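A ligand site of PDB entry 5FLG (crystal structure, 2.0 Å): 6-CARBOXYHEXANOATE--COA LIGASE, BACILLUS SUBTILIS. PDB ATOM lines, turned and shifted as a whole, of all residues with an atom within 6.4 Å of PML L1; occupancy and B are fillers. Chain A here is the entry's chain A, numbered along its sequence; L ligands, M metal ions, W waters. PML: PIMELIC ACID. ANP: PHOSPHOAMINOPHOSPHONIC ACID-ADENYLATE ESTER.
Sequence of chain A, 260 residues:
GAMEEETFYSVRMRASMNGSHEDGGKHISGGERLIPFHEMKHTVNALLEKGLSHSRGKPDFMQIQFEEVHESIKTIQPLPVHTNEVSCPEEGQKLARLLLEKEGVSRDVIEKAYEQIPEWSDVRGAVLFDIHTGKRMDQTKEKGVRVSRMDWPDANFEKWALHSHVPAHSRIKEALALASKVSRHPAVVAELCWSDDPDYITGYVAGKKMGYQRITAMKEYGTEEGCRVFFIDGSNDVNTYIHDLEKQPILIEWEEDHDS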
ATOM      1  N   SER A 170      11.234 -14.091  24.311  1.00  0.00           N
ATOM      2  CA  SER A 170       9.844 -14.463  24.216  1.00  0.00           C
ATOM      3  C   SER A 170       8.900 -13.266  24.295  1.00  0.00           C
ATOM      4  O   SER A 170       7.824 -13.292  23.697  1.00  0.00           O
ATOM      5  CB  SER A 170       9.491 -15.413  25.336  1.00  0.00           C
ATOM      6  OG  SER A 170      10.250 -16.581  25.216  1.00  0.00           O
ATOM      7  N   ARG A 171       9.179 -12.350  25.215  1.00  0.00           N
ATOM      8  CA  ARG A 171       8.389 -11.134  25.367  1.00  0.00           C
ATOM      9  C   ARG A 171       8.200 -10.469  23.990  1.00  0.00           C
ATOM     10  O   ARG A 171       7.125  -9.887  23.713  1.00  0.00           O
ATOM     11  CB  ARG A 171       9.099 -10.145  26.314  1.00  0.00           C
ATOM     12  CG  ARG A 171       8.755 -10.305  27.779  1.00  0.00           C
ATOM     13  CD  ARG A 171       9.172  -9.070  28.567  1.00  0.00           C
ATOM     14  NE  ARG A 171       8.755  -9.112  29.977  1.00  0.00           N
ATOM     15  CZ  ARG A 171       9.575  -9.442  30.974  1.00  0.00           C
ATOM     16  NH1 ARG A 171      10.802  -9.854  30.695  1.00  0.00           N
ATOM     17  NH2 ARG A 171       9.158  -9.447  32.232  1.00  0.00           N
ATOM     18  N   ILE A 172       9.292 -10.379  23.228  1.00  0.00           N
ATOM     19  CA  ILE A 172       9.258  -9.602  21.981  1.00  0.00           C
ATOM     20  C   ILE A 172       8.498 -10.375  20.918  1.00  0.00           C
ATOM     21  O   ILE A 172       7.603  -9.824  20.245  1.00  0.00           O
ATOM     22  CB  ILE A 172      10.665  -9.265  21.479  1.00  0.00           C
ATOM     23  CG1 ILE A 172      11.357  -8.317  22.445  1.00  0.00           C
ATOM     24  CG2 ILE A 172      10.608  -8.674  20.068  1.00  0.00           C
ATOM     25  CD1 ILE A 172      12.868  -8.267  22.263  1.00  0.00           C
ATOM     26  N   GLU A 174       6.026 -12.438  21.508  1.00  0.00           N
ATOM     27  CA  GLU A 174       4.638 -12.318  21.863  1.00  0.00           C
ATOM     28  C   GLU A 174       4.076 -10.940  21.546  1.00  0.00           C
ATOM     29  O   GLU A 174       3.049 -10.841  20.899  1.00  0.00           O
ATOM     30  CB  GLU A 174       4.413 -12.689  23.343  1.00  0.00           C
ATOM     31  CG  GLU A 174       4.553 -14.188  23.611  1.00  0.00           C
ATOM     32  CD  GLU A 174       4.901 -14.553  25.077  1.00  0.00           C
ATOM     33  OE1 GLU A 174       4.939 -13.684  25.969  1.00  0.00           O
ATOM     34  OE2 GLU A 174       5.135 -15.747  25.331  1.00  0.00           O
ATOM     35  N   ALA A 175       4.811  -9.893  21.886  1.00  0.00           N
ATOM     36  CA  ALA A 175       4.326  -8.571  21.701  1.00  0.00           C
ATOM     37  C   ALA A 175       4.215  -8.256  20.228  1.00  0.00           C
ATOM     38  O   ALA A 175       3.266  -7.582  19.789  1.00  0.00           O
ATOM     39  CB  ALA A 175       5.246  -7.586  22.376  1.00  0.00           C
ATOM     40  N   LEU A 176       5.249  -8.610  19.465  1.00  0.00           N
ATOM     41  CA  LEU A 176       5.255  -8.285  18.043  1.00  0.00           C
ATOM     42  C   LEU A 176       4.194  -9.104  17.297  1.00  0.00           C
ATOM     43  O   LEU A 176       3.576  -8.616  16.321  1.00  0.00           O
ATOM     44  CB  LEU A 176       6.660  -8.444  17.453  1.00  0.00           C
ATOM     45  CG  LEU A 176       6.899  -8.015  15.996  1.00  0.00           C
ATOM     46  CD1 LEU A 176       6.329  -6.628  15.661  1.00  0.00           C
ATOM     47  CD2 LEU A 176       8.377  -8.061  15.700  1.00  0.00           C
ATOM     48  N   CYS A 193       1.633   0.523  24.366  1.00  0.00           N
ATOM     49  CA  CYS A 193       1.850  -0.625  25.227  1.00  0.00           C
ATOM     50  C   CYS A 193       3.059  -0.441  26.126  1.00  0.00           C
ATOM     51  O   CYS A 193       4.121   0.035  25.689  1.00  0.00           O
ATOM     52  CB  CYS A 193       2.048  -1.876  24.408  1.00  0.00           C
ATOM     53  SG  CYS A 193       2.680  -3.289  25.389  1.00  0.00           S
ATOM     54  N   TRP A 194       2.911  -0.787  27.400  1.00  0.00           N
ATOM     55  CA  TRP A 194       4.079  -1.192  28.202  1.00  0.00           C
ATOM     56  C   TRP A 194       3.674  -2.191  29.260  1.00  0.00           C
ATOM     57  O   TRP A 194       2.492  -2.484  29.444  1.00  0.00           O
ATOM     58  CB  TRP A 194       4.830   0.043  28.774  1.00  0.00           C
ATOM     59  CG  TRP A 194       4.049   0.867  29.779  1.00  0.00           C
ATOM     60  CD1 TRP A 194       4.040   0.716  31.134  1.00  0.00           C
ATOM     61  CD2 TRP A 194       3.242   2.017  29.498  1.00  0.00           C
ATOM     62  NE1 TRP A 194       3.158   1.625  31.699  1.00  0.00           N
ATOM     63  CE2 TRP A 194       2.756   2.494  30.728  1.00  0.00           C
ATOM     64  CE3 TRP A 194       2.897   2.693  28.330  1.00  0.00           C
ATOM     65  CZ2 TRP A 194       1.863   3.574  30.811  1.00  0.00           C
ATOM     66  CZ3 TRP A 194       2.078   3.787  28.412  1.00  0.00           C
ATOM     67  CH2 TRP A 194       1.567   4.219  29.645  1.00  0.00           C
ATOM     68  N   SER A 195       4.682  -2.859  29.821  1.00  0.00           N
ATOM     69  CA  SER A 195       4.472  -4.044  30.592  1.00  0.00           C
ATOM     70  C   SER A 195       3.897  -3.712  31.957  1.00  0.00           C
ATOM     71  O   SER A 195       4.270  -2.706  32.562  1.00  0.00           O
ATOM     72  CB  SER A 195       5.830  -4.787  30.803  1.00  0.00           C
ATOM     73  OG  SER A 195       5.569  -6.060  31.374  1.00  0.00           O
ATOM     74  N   ASP A 196       3.113  -4.616  32.501  1.00  0.00           N
ATOM     75  CA  ASP A 196       2.766  -4.573  33.930  1.00  0.00           C
ATOM     76  C   ASP A 196       3.746  -5.435  34.769  1.00  0.00           C
ATOM     77  O   ASP A 196       3.551  -5.567  35.977  1.00  0.00           O
ATOM     78  CB  ASP A 196       1.330  -5.033  34.169  1.00  0.00           C
ATOM     79  CG  ASP A 196       1.046  -6.435  33.578  1.00  0.00           C
ATOM     80  OD1 ASP A 196       1.866  -6.906  32.756  1.00  0.00           O
ATOM     81  OD2 ASP A 196       0.017  -7.061  33.953  1.00  0.00           O
ATOM     82  N   ASP A 197       4.846  -5.877  34.197  1.00  0.00           N
ATOM     83  CA  ASP A 197       5.896  -6.580  34.995  1.00  0.00           C
ATOM     84  C   ASP A 197       6.828  -5.568  35.722  1.00  0.00           C
ATOM     85  O   ASP A 197       7.308  -4.625  35.107  1.00  0.00           O
ATOM     86  CB  ASP A 197       6.768  -7.438  34.091  1.00  0.00           C
ATOM     87  CG  ASP A 197       5.986  -8.523  33.329  1.00  0.00           C
ATOM     88  OD1 ASP A 197       4.753  -8.707  33.498  1.00  0.00           O
ATOM     89  OD2 ASP A 197       6.625  -9.157  32.453  1.00  0.00           O
ATOM     90  N   TYR A 200      10.528  -5.162  33.772  1.00  0.00           N
ATOM     91  CA  TYR A 200      10.679  -4.899  32.333  1.00  0.00           C
ATOM     92  C   TYR A 200      10.057  -3.570  31.926  1.00  0.00           C
ATOM     93  O   TYR A 200       8.836  -3.366  32.098  1.00  0.00           O
ATOM     94  CB  TYR A 200      10.051  -6.029  31.559  1.00  0.00           C
ATOM     95  CG  TYR A 200      10.511  -6.095  30.135  1.00  0.00           C
ATOM     96  CD1 TYR A 200      11.741  -6.651  29.798  1.00  0.00           C
ATOM     97  CD2 TYR A 200       9.753  -5.499  29.122  1.00  0.00           C
ATOM     98  CE1 TYR A 200      12.173  -6.715  28.489  1.00  0.00           C
ATOM     99  CE2 TYR A 200      10.207  -5.481  27.813  1.00  0.00           C
ATOM    100  CZ  TYR A 200      11.408  -6.094  27.491  1.00  0.00           C
ATOM    101  OH  TYR A 200      11.800  -6.156  26.179  1.00  0.00           O
ATOM    102  N   THR A 202      10.764  -1.664  28.962  1.00  0.00           N
ATOM    103  CA  THR A 202      10.560  -1.399  27.534  1.00  0.00           C
ATOM    104  C   THR A 202       9.126  -1.572  27.125  1.00  0.00           C
ATOM    105  O   THR A 202       8.406  -2.409  27.675  1.00  0.00           O
ATOM    106  CB  THR A 202      11.411  -2.304  26.684  1.00  0.00           C
ATOM    107  OG1 THR A 202      12.783  -2.124  27.027  1.00  0.00           O
ATOM    108  CG2 THR A 202      11.226  -2.004  25.213  1.00  0.00           C
ATOM    109  N   GLY A 203       8.646  -0.621  26.318  1.00  0.00           N
ATOM    110  CA  GLY A 203       7.327  -0.715  25.730  1.00  0.00           C
ATOM    111  C   GLY A 203       7.374  -0.344  24.266  1.00  0.00           C
ATOM    112  O   GLY A 203       8.448  -0.398  23.648  1.00  0.00           O
ATOM    113  N   TYR A 204       6.222   0.034  23.683  1.00  0.00           N
ATOM    114  CA  TYR A 204       6.202   0.346  22.282  1.00  0.00           C
ATOM    115  C   TYR A 204       4.920   1.084  21.893  1.00  0.00           C
ATOM    116  O   TYR A 204       3.984   1.196  22.663  1.00  0.00           O
ATOM    117  CB  TYR A 204       6.321  -0.903  21.411  1.00  0.00           C
ATOM    118  CG  TYR A 204       5.102  -1.857  21.440  1.00  0.00           C
ATOM    119  CD1 TYR A 204       4.019  -1.654  20.606  1.00  0.00           C
ATOM    120  CD2 TYR A 204       5.075  -2.950  22.302  1.00  0.00           C
ATOM    121  CE1 TYR A 204       2.950  -2.484  20.628  1.00  0.00           C
ATOM    122  CE2 TYR A 204       4.038  -3.852  22.247  1.00  0.00           C
ATOM    123  CZ  TYR A 204       2.932  -3.562  21.457  1.00  0.00           C
ATOM    124  OH  TYR A 204       1.866  -4.420  21.389  1.00  0.00           O
ATOM    125  N   TYR A 212       6.487  -1.029  14.280  1.00  0.00           N
ATOM    126  CA  TYR A 212       6.640  -1.362  15.723  1.00  0.00           C
ATOM    127  C   TYR A 212       7.816  -0.595  16.287  1.00  0.00           C
ATOM    128  O   TYR A 212       8.983  -0.914  16.027  1.00  0.00           O
ATOM    129  CB  TYR A 212       6.888  -2.854  15.879  1.00  0.00           C
ATOM    130  CG  TYR A 212       6.977  -3.399  17.316  1.00  0.00           C
ATOM    131  CD1 TYR A 212       5.829  -3.770  17.991  1.00  0.00           C
ATOM    132  CD2 TYR A 212       8.176  -3.835  17.817  1.00  0.00           C
ATOM    133  CE1 TYR A 212       5.873  -4.424  19.200  1.00  0.00           C
ATOM    134  CE2 TYR A 212       8.260  -4.453  19.070  1.00  0.00           C
ATOM    135  CZ  TYR A 212       7.098  -4.744  19.748  1.00  0.00           C
ATOM    136  OH  TYR A 212       7.125  -5.312  20.992  1.00  0.00           O
ATOM    137  N   ARG A 214       9.803   0.364  19.249  1.00  0.00           N
ATOM    138  CA  ARG A 214      10.124   0.049  20.629  1.00  0.00           C
ATOM    139  C   ARG A 214      10.679   1.283  21.315  1.00  0.00           C
ATOM    140  O   ARG A 214      11.492   1.981  20.752  1.00  0.00           O
ATOM    141  CB  ARG A 214      11.185  -1.070  20.674  1.00  0.00           C
ATOM    142  CG  ARG A 214      10.791  -2.286  19.897  1.00  0.00           C
ATOM    143  CD  ARG A 214      11.873  -3.344  19.884  1.00  0.00           C
ATOM    144  NE  ARG A 214      12.060  -3.908  21.195  1.00  0.00           N
ATOM    145  CZ  ARG A 214      13.235  -3.997  21.817  1.00  0.00           C
ATOM    146  NH1 ARG A 214      14.317  -3.503  21.257  1.00  0.00           N
ATOM    147  NH2 ARG A 214      13.317  -4.573  23.001  1.00  0.00           N
ATOM    148  N   ARG A 228      -2.133  -1.204  27.780  1.00  0.00           N
ATOM    149  CA  ARG A 228      -2.377  -1.698  26.464  1.00  0.00           C
ATOM    150  C   ARG A 228      -3.642  -0.959  25.977  1.00  0.00           C
ATOM    151  O   ARG A 228      -4.749  -1.280  26.382  1.00  0.00           O
ATOM    152  CB  ARG A 228      -2.611  -3.210  26.503  1.00  0.00           C
ATOM    153  CG  ARG A 228      -2.262  -3.940  25.225  1.00  0.00           C
ATOM    154  CD  ARG A 228      -0.781  -3.934  25.054  1.00  0.00           C
ATOM    155  NE  ARG A 228      -0.225  -4.878  24.079  1.00  0.00           N
ATOM    156  CZ  ARG A 228       0.567  -5.895  24.401  1.00  0.00           C
ATOM    157  NH1 ARG A 228       0.631  -6.345  25.661  1.00  0.00           N
ATOM    158  NH2 ARG A 228       1.327  -6.435  23.468  1.00  0.00           N
HETATM  159  C1  PML L   1       9.457  -5.306  23.468  1.00  0.00           C
HETATM  160  O11 PML L   1       9.502  -5.013  22.233  1.00  0.00           O
HETATM  161  O12 PML L   1      10.533  -5.567  24.114  1.00  0.00           O
HETATM  162  C2  PML L   1       8.170  -4.922  24.218  1.00  0.00           C
HETATM  163  C3  PML L   1       7.465  -6.007  25.012  1.00  0.00           C
HETATM  164  C4  PML L   1       6.721  -5.493  26.261  1.00  0.00           C
HETATM  165  C5  PML L   1       5.281  -5.932  26.374  1.00  0.00           C
HETATM  166  C6  PML L   1       4.898  -6.514  27.739  1.00  0.00           C
HETATM  167  C7  PML L   1       5.729  -7.745  28.097  1.00  0.00           C
HETATM  168  O71 PML L   1       5.699  -8.735  27.339  1.00  0.00           O
HETATM  169  O72 PML L   1       6.331  -7.773  29.204  1.00  0.00           O
HETATM  170  PG  ANP L   2       2.644 -12.036  30.947  1.00  0.00           P
HETATM  171  O1G ANP L   2       2.750 -13.381  31.612  1.00  0.00           O
HETATM  172  O2G ANP L   2       3.478 -10.991  31.641  1.00  0.00           O
HETATM  173  O3G ANP L   2       2.872 -12.016  29.466  1.00  0.00           O
HETATM  174  PB  ANP L   2       0.220 -10.522  30.145  1.00  0.00           P
HETATM  175  O1B ANP L   2       0.408 -11.026  28.749  1.00  0.00           O
HETATM  176  O2B ANP L   2      -1.107 -10.351  30.783  1.00  0.00           O
HETATM  177  N3B ANP L   2       1.009 -11.610  31.223  1.00  0.00           N
HETATM  178  PA  ANP L   2       2.112  -8.510  29.318  1.00  0.00           P
HETATM  179  O1A ANP L   2       3.159  -7.808  30.038  1.00  0.00           O
HETATM  180  O2A ANP L   2       2.397  -9.495  28.222  1.00  0.00           O
HETATM  181  O3A ANP L   2       1.020  -9.130  30.337  1.00  0.00           O
HETATM  182  O5' ANP L   2       1.184  -7.296  28.682  1.00  0.00           O
HETATM  183  C5' ANP L   2       1.064  -6.067  29.340  1.00  0.00           C
HETATM  184  C4' ANP L   2      -0.414  -5.641  29.357  1.00  0.00           C
HETATM  185  O4' ANP L   2      -0.887  -5.612  28.009  1.00  0.00           O
HETATM  186  C3' ANP L   2      -1.281  -6.628  30.113  1.00  0.00           C
HETATM  187  O3' ANP L   2      -1.436  -6.245  31.477  1.00  0.00           O
HETATM  188  C2' ANP L   2      -2.606  -6.486  29.409  1.00  0.00           C
HETATM  189  O2' ANP L   2      -3.260  -5.316  29.898  1.00  0.00           O
HETATM  190  C1' ANP L   2      -2.166  -6.253  27.995  1.00  0.00           C
HETATM  191  N9  ANP L   2      -2.155  -7.534  27.287  1.00  0.00           N
HETATM  192  C8  ANP L   2      -1.242  -8.565  27.401  1.00  0.00           C
HETATM  193  N7  ANP L   2      -1.542  -9.548  26.515  1.00  0.00           N
HETATM  194  C5  ANP L   2      -2.676  -9.164  25.859  1.00  0.00           C
HETATM  195  C6  ANP L   2      -3.576  -9.716  24.836  1.00  0.00           C
HETATM  196  N6  ANP L   2      -3.374 -10.930  24.302  1.00  0.00           N
HETATM  197  N1  ANP L   2      -4.632  -8.981  24.425  1.00  0.00           N
HETATM  198  C2  ANP L   2      -4.885  -7.786  24.966  1.00  0.00           C
HETATM  199  N3  ANP L   2      -4.105  -7.162  25.851  1.00  0.00           N
HETATM  200  C4  ANP L   2      -3.073  -7.853  26.395  1.00  0.00           C
HETATM  201 MG    MG M   1       2.009 -11.351  27.640  1.00  0.00          MG
HETATM  202 MG    MG M   2       2.843  -8.889  32.360  1.00  0.00          MG
HETATM  203  O   HOH W   1       3.679 -11.431  26.583  1.00  0.00           O
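An oxygen (O11) of PML L1 is in salt-bridge range of the guanidinium group of Arg 214 (3.0 Å).
An oxygen (O1A) of ANP L2 sits close to the side-chain hydroxyl (OG) of Ser 195, at 3.3 Å.
NE of Arg 171 lies within salt-bridge range of O72 of PML L1.
The side-chain hydroxyl (OH) of Tyr 200 lies within hydrogen-bond range of an oxygen (O12) of PML L1.
O72 of PML L1 lies within hydrogen-bond range of OG of Ser 195 (2.9 Å).
The guanidinium group (NH1) of Arg 228 lies within hydrogen-bond range of an oxygen (O4') of ANP L2 (2.9 Å).
An oxygen (O11) of PML L1 lies within hydrogen-bond range of the side-chain hydroxyl (OH) of Tyr 212.
The side-chain hydroxyl of Ser 195 sits at hydrogen-bond distance from the backbone NH of Asp 197 (2.9 Å).
The side-chain sulfur (SG) of Cys 193 sits close to the guanidinium group (NE) of Arg 228, 3.6 Å away.
O of Cys 193 lies within hydrogen-bond range of N of Tyr 204 (2.9 Å).
OD2 of Asp 197 is in salt-bridge range of NH2 of Arg 171, 2.6 Å away.
Ile 172 touches PML L1 (CG1 to O12, 3.3 Å).
Ala 175 touches PML L1 (CB to C3, 3.8 Å).
Cys 193 touches PML L1.
Asp 197 touches PML L1.
Thr 202 touches PML L1 (O to C4, 3.8 Å).
Of the 18 residues printed, 10 come within 4 Å of PML L1.
Water W1 lies within hydrogen-bond range of the side-chain carboxylate (OE1) of Glu 174 (2.7 Å) and an oxygen (O71) of PML L1 (3.5 Å).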
